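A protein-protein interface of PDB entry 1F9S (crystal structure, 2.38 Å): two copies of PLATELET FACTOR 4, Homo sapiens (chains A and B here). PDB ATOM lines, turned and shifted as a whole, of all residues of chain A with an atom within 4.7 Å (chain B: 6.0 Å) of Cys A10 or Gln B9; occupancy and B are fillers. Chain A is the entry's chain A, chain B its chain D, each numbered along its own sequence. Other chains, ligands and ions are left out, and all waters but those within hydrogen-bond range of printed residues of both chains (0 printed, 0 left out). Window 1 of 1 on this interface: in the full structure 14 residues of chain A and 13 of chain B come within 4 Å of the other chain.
Among the printed residues, pairs that only touch across the chains: Leu A11 with Leu B8, Leu A11 with Leu B11, Cys A12 with Asp B7 and Leu A11 with Asp B7.
The backbone NH (N) of Cys A10 is in hydrogen-bond range of the backbone carbonyl oxygen (O) of His A35 (3.2 Å). The side-chain sulfur (SG) of Cys A36 forms a disulfide with the side-chain sulfur (SG) of Cys A10, 2.0 Å away. OE1 of Gln A40 is in hydrogen-bond range of N of Cys A12. The backbone NH of Cys B10 lies within hydrogen-bond range of the backbone carbonyl oxygen of His B35 (3.4 Å). The side-chain sulfur (SG) of Cys B10 forms a disulfide with the side-chain sulfur (SG) of Cys B36, at 2.0 Å. N of Leu B11 sits at hydrogen-bond distance from OE1 of Gln B40 (3.3 Å).
The side-chain amide nitrogen (NE2) of Gln A9 sits close to the side-chain amide oxygen (OE1) of Gln B9 (3.3 Å). The side-chain amide nitrogen (NE2) of Gln A9 is in hydrogen-bond range of the backbone carbonyl oxygen (O) of Cys B10 (2.5 Å). The backbone NH (N) of Gln A9 is in hydrogen-bond range of the backbone carbonyl oxygen (O) of Leu B11, at 2.9 Å. The backbone carbonyl oxygen of Cys A10 is in hydrogen-bond range of the side-chain amide nitrogen of Gln B9. N of Gln B9 is in hydrogen-bond range of O of Leu A11, 3.0 Å away.
Printed residues of chain B within 4 Å of Gln A9: Gln B9 (3.2 Å), Cys B10 (2.5 Å) and Leu B11 (2.9 Å). Of the printed residues of chain B, Leu A11 touches Asp B7, Leu B8, Gln B9 and Leu B11. Of the printed residues of chain B, Cys A12 touches Asp B7. Printed residues of chain A within 4 Å of Leu B8: Leu A11 (3.0 Å). Of chain A, only Gln A9, Cys A10 and Leu A11 come within 4 Å of Gln B9. Of the printed residues of chain A, Cys B10 touches Gln A9. Cys B36 touches none of the printed residues of chain A. The nearest residue of chain B that does not touch Cys A10 is Cys B10 (4.2 Å).
Hydrophobic or aromatic side chains of chain B that line the printed part of chain A: Leu B8 and Leu B11. Of the 8 printed residues of chain A, 4 touch a printed residue of chain B. Printed residues of chain A that touch a printed residue of chain B: Gln A9, Cys A10, Leu A11 and Cys A12. Hydrophobic or aromatic side chains of chain A within 4 Å of the printed part of chain B: Leu A11. Among the printed residues, 9 pairs touch across the chains. Among the printed residues, no Asp or Glu carboxylate lies within 4 Å of a Lys or Arg side-chain nitrogen of the other chain.
Gln B9 touches its own counterpart, Gln A9. Gln A9 touches Cys B10, and with the chains exchanged Cys A10 touches Gln B9. Gln A9 touches Leu B11, and with the chains exchanged Leu A11 touches Gln B9. Leu A11 touches its own counterpart, Leu B11. Of the 9 pairs that touch across the chains among the printed residues, 6 have their exchanged pair printed and touching as well.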
ATOM      1  N   GLN A   9      -4.489  24.458  -7.569  1.00  0.00           N
ATOM      2  CA  GLN A   9      -3.486  23.510  -7.139  1.00  0.00           C
ATOM      3  C   GLN A   9      -2.406  23.499  -8.221  1.00  0.00           C
ATOM      4  O   GLN A   9      -2.600  24.084  -9.284  1.00  0.00           O
ATOM      5  CB  GLN A   9      -4.117  22.122  -6.965  1.00  0.00           C
ATOM      6  CG  GLN A   9      -4.350  21.323  -8.234  1.00  0.00           C
ATOM      7  CD  GLN A   9      -4.921  19.945  -7.943  1.00  0.00           C
ATOM      8  OE1 GLN A   9      -4.671  19.375  -6.889  1.00  0.00           O
ATOM      9  NE2 GLN A   9      -5.671  19.397  -8.891  1.00  0.00           N
ATOM     10  N   CYS A  10      -1.270  22.858  -7.969  1.00  0.00           N
ATOM     11  CA  CYS A  10      -0.229  22.838  -8.988  1.00  0.00           C
ATOM     12  C   CYS A  10      -0.759  22.143 -10.225  1.00  0.00           C
ATOM     13  O   CYS A  10      -1.451  21.128 -10.145  1.00  0.00           O
ATOM     14  CB  CYS A  10       1.019  22.100  -8.511  1.00  0.00           C
ATOM     15  SG  CYS A  10       1.686  22.656  -6.913  1.00  0.00           S
ATOM     16  N   LEU A  11      -0.445  22.712 -11.369  1.00  0.00           N
ATOM     17  CA  LEU A  11      -0.852  22.157 -12.635  1.00  0.00           C
ATOM     18  C   LEU A  11       0.073  20.955 -12.813  1.00  0.00           C
ATOM     19  O   LEU A  11      -0.349  19.842 -13.112  1.00  0.00           O
ATOM     20  CB  LEU A  11      -0.603  23.209 -13.709  1.00  0.00           C
ATOM     21  CG  LEU A  11      -1.483  23.260 -14.950  1.00  0.00           C
ATOM     22  CD1 LEU A  11      -1.054  24.457 -15.778  1.00  0.00           C
ATOM     23  CD2 LEU A  11      -1.360  21.981 -15.748  1.00  0.00           C
ATOM     24  N   CYS A  12       1.356  21.207 -12.602  1.00  0.00           N
ATOM     25  CA  CYS A  12       2.385  20.191 -12.712  1.00  0.00           C
ATOM     26  C   CYS A  12       2.244  19.166 -11.599  1.00  0.00           C
ATOM     27  O   CYS A  12       1.842  19.509 -10.493  1.00  0.00           O
ATOM     28  CB  CYS A  12       3.751  20.872 -12.637  1.00  0.00           C
ATOM     29  SG  CYS A  12       4.093  21.855 -14.127  1.00  0.00           S
ATOM     30  N   HIS A  35      -1.699  28.794  -5.077  1.00  0.00           N
ATOM     31  CA  HIS A  35      -2.011  27.712  -5.992  1.00  0.00           C
ATOM     32  C   HIS A  35      -0.961  26.617  -5.949  1.00  0.00           C
ATOM     33  O   HIS A  35      -1.268  25.438  -6.114  1.00  0.00           O
ATOM     34  CB  HIS A  35      -2.108  28.270  -7.411  1.00  0.00           C
ATOM     35  CG  HIS A  35      -0.844  28.921  -7.880  1.00  0.00           C
ATOM     36  ND1 HIS A  35       0.245  28.191  -8.323  1.00  0.00           N
ATOM     37  CD2 HIS A  35      -0.467  30.218  -7.917  1.00  0.00           C
ATOM     38  CE1 HIS A  35       1.236  29.019  -8.610  1.00  0.00           C
ATOM     39  NE2 HIS A  35       0.828  30.250  -8.371  1.00  0.00           N
ATOM     40  N   CYS A  36       0.281  27.003  -5.719  1.00  0.00           N
ATOM     41  CA  CYS A  36       1.337  26.024  -5.710  1.00  0.00           C
ATOM     42  C   CYS A  36       2.560  26.528  -4.938  1.00  0.00           C
ATOM     43  O   CYS A  36       3.063  27.620  -5.195  1.00  0.00           O
ATOM     44  CB  CYS A  36       1.689  25.682  -7.161  1.00  0.00           C
ATOM     45  SG  CYS A  36       2.814  24.278  -7.366  1.00  0.00           S
ATOM     46  N   PRO A  37       3.053  25.725  -3.980  1.00  0.00           N
ATOM     47  CA  PRO A  37       4.208  26.040  -3.138  1.00  0.00           C
ATOM     48  C   PRO A  37       5.521  26.239  -3.887  1.00  0.00           C
ATOM     49  O   PRO A  37       6.452  26.855  -3.363  1.00  0.00           O
ATOM     50  CB  PRO A  37       4.251  24.857  -2.173  1.00  0.00           C
ATOM     51  CG  PRO A  37       3.744  23.736  -3.015  1.00  0.00           C
ATOM     52  CD  PRO A  37       2.554  24.373  -3.677  1.00  0.00           C
ATOM     53  N   GLN A  40       6.674  26.814 -11.418  1.00  0.00           N
ATOM     54  CA  GLN A  40       6.421  25.772 -12.409  1.00  0.00           C
ATOM     55  C   GLN A  40       6.877  26.154 -13.820  1.00  0.00           C
ATOM     56  O   GLN A  40       6.785  27.317 -14.224  1.00  0.00           O
ATOM     57  CB  GLN A  40       4.936  25.408 -12.426  1.00  0.00           C
ATOM     58  CG  GLN A  40       4.375  25.063 -11.073  1.00  0.00           C
ATOM     59  CD  GLN A  40       2.868  24.911 -11.097  1.00  0.00           C
ATOM     60  OE1 GLN A  40       2.336  23.843 -11.408  1.00  0.00           O
ATOM     61  NE2 GLN A  40       2.165  25.995 -10.781  1.00  0.00           N
ATOM     62  N   GLY B   6       0.570  11.556 -18.174  1.00  0.00           N
ATOM     63  CA  GLY B   6       0.388  13.034 -18.173  1.00  0.00           C
ATOM     64  C   GLY B   6       1.087  13.713 -17.010  1.00  0.00           C
ATOM     65  O   GLY B   6       0.967  13.280 -15.855  1.00  0.00           O
ATOM     66  N   ASP B   7       1.820  14.781 -17.317  1.00  0.00           N
ATOM     67  CA  ASP B   7       2.554  15.537 -16.303  1.00  0.00           C
ATOM     68  C   ASP B   7       1.652  16.530 -15.611  1.00  0.00           C
ATOM     69  O   ASP B   7       1.991  17.062 -14.549  1.00  0.00           O
ATOM     70  CB  ASP B   7       3.716  16.304 -16.936  1.00  0.00           C
ATOM     71  CG  ASP B   7       4.976  15.480 -17.029  1.00  0.00           C
ATOM     72  OD1 ASP B   7       6.015  16.026 -17.460  1.00  0.00           O
ATOM     73  OD2 ASP B   7       4.929  14.289 -16.663  1.00  0.00           O
ATOM     74  N   LEU B   8       0.498  16.779 -16.213  1.00  0.00           N
ATOM     75  CA  LEU B   8      -0.413  17.752 -15.656  1.00  0.00           C
ATOM     76  C   LEU B   8      -1.734  17.188 -15.159  1.00  0.00           C
ATOM     77  O   LEU B   8      -2.235  16.170 -15.641  1.00  0.00           O
ATOM     78  CB  LEU B   8      -0.687  18.848 -16.687  1.00  0.00           C
ATOM     79  CG  LEU B   8       0.453  19.689 -17.269  1.00  0.00           C
ATOM     80  CD1 LEU B   8       1.451  18.840 -18.026  1.00  0.00           C
ATOM     81  CD2 LEU B   8      -0.159  20.685 -18.221  1.00  0.00           C
ATOM     82  N   GLN B   9      -2.290  17.885 -14.181  1.00  0.00           N
ATOM     83  CA  GLN B   9      -3.555  17.530 -13.585  1.00  0.00           C
ATOM     84  C   GLN B   9      -4.413  18.780 -13.702  1.00  0.00           C
ATOM     85  O   GLN B   9      -4.009  19.772 -14.317  1.00  0.00           O
ATOM     86  CB  GLN B   9      -3.354  17.172 -12.113  1.00  0.00           C
ATOM     87  CG  GLN B   9      -3.022  18.352 -11.226  1.00  0.00           C
ATOM     88  CD  GLN B   9      -2.902  17.953  -9.774  1.00  0.00           C
ATOM     89  OE1 GLN B   9      -3.533  16.991  -9.342  1.00  0.00           O
ATOM     90  NE2 GLN B   9      -2.106  18.696  -9.006  1.00  0.00           N
ATOM     91  N   CYS B  10      -5.597  18.735 -13.111  1.00  0.00           N
ATOM     92  CA  CYS B  10      -6.486  19.881 -13.154  1.00  0.00           C
ATOM     93  C   CYS B  10      -5.998  20.934 -12.175  1.00  0.00           C
ATOM     94  O   CYS B  10      -5.552  20.615 -11.068  1.00  0.00           O
ATOM     95  CB  CYS B  10      -7.902  19.478 -12.765  1.00  0.00           C
ATOM     96  SG  CYS B  10      -8.655  18.158 -13.752  1.00  0.00           S
ATOM     97  N   LEU B  11      -6.090  22.191 -12.589  1.00  0.00           N
ATOM     98  CA  LEU B  11      -5.670  23.306 -11.754  1.00  0.00           C
ATOM     99  C   LEU B  11      -6.739  23.463 -10.670  1.00  0.00           C
ATOM    100  O   LEU B  11      -6.434  23.549  -9.476  1.00  0.00           O
ATOM    101  CB  LEU B  11      -5.578  24.567 -12.612  1.00  0.00           C
ATOM    102  CG  LEU B  11      -4.587  25.656 -12.199  1.00  0.00           C
ATOM    103  CD1 LEU B  11      -3.145  25.229 -12.505  1.00  0.00           C
ATOM    104  CD2 LEU B  11      -4.924  26.919 -12.966  1.00  0.00           C
ATOM    105  N   HIS B  35      -5.133  16.883 -19.672  1.00  0.00           N
ATOM    106  CA  HIS B  35      -4.688  17.536 -18.446  1.00  0.00           C
ATOM    107  C   HIS B  35      -5.811  17.524 -17.435  1.00  0.00           C
ATOM    108  O   HIS B  35      -5.570  17.504 -16.237  1.00  0.00           O
ATOM    109  CB  HIS B  35      -4.324  18.993 -18.737  1.00  0.00           C
ATOM    110  CG  HIS B  35      -5.459  19.787 -19.318  1.00  0.00           C
ATOM    111  ND1 HIS B  35      -6.016  19.497 -20.549  1.00  0.00           N
ATOM    112  CD2 HIS B  35      -6.166  20.831 -18.824  1.00  0.00           C
ATOM    113  CE1 HIS B  35      -7.018  20.330 -20.783  1.00  0.00           C
ATOM    114  NE2 HIS B  35      -7.130  21.147 -19.752  1.00  0.00           N
ATOM    115  N   CYS B  36      -7.040  17.537 -17.936  1.00  0.00           N
ATOM    116  CA  CYS B  36      -8.209  17.592 -17.081  1.00  0.00           C
ATOM    117  C   CYS B  36      -9.466  17.113 -17.820  1.00  0.00           C
ATOM    118  O   CYS B  36      -9.810  17.628 -18.886  1.00  0.00           O
ATOM    119  CB  CYS B  36      -8.393  19.032 -16.594  1.00  0.00           C
ATOM    120  SG  CYS B  36      -9.593  19.150 -15.246  1.00  0.00           S
ATOM    121  N   GLN B  40     -12.731  24.080 -17.316  1.00  0.00           N
ATOM    122  CA  GLN B  40     -12.514  24.839 -16.088  1.00  0.00           C
ATOM    123  C   GLN B  40     -12.772  26.328 -16.299  1.00  0.00           C
ATOM    124  O   GLN B  40     -12.485  26.858 -17.363  1.00  0.00           O
ATOM    125  CB  GLN B  40     -11.095  24.615 -15.592  1.00  0.00           C
ATOM    126  CG  GLN B  40     -10.652  23.163 -15.633  1.00  0.00           C
ATOM    127  CD  GLN B  40      -9.214  22.998 -15.182  1.00  0.00           C
ATOM    128  OE1 GLN B  40      -8.933  22.937 -13.982  1.00  0.00           O
ATOM    129  NE2 GLN B  40      -8.291  22.943 -16.144  1.00  0.00           N
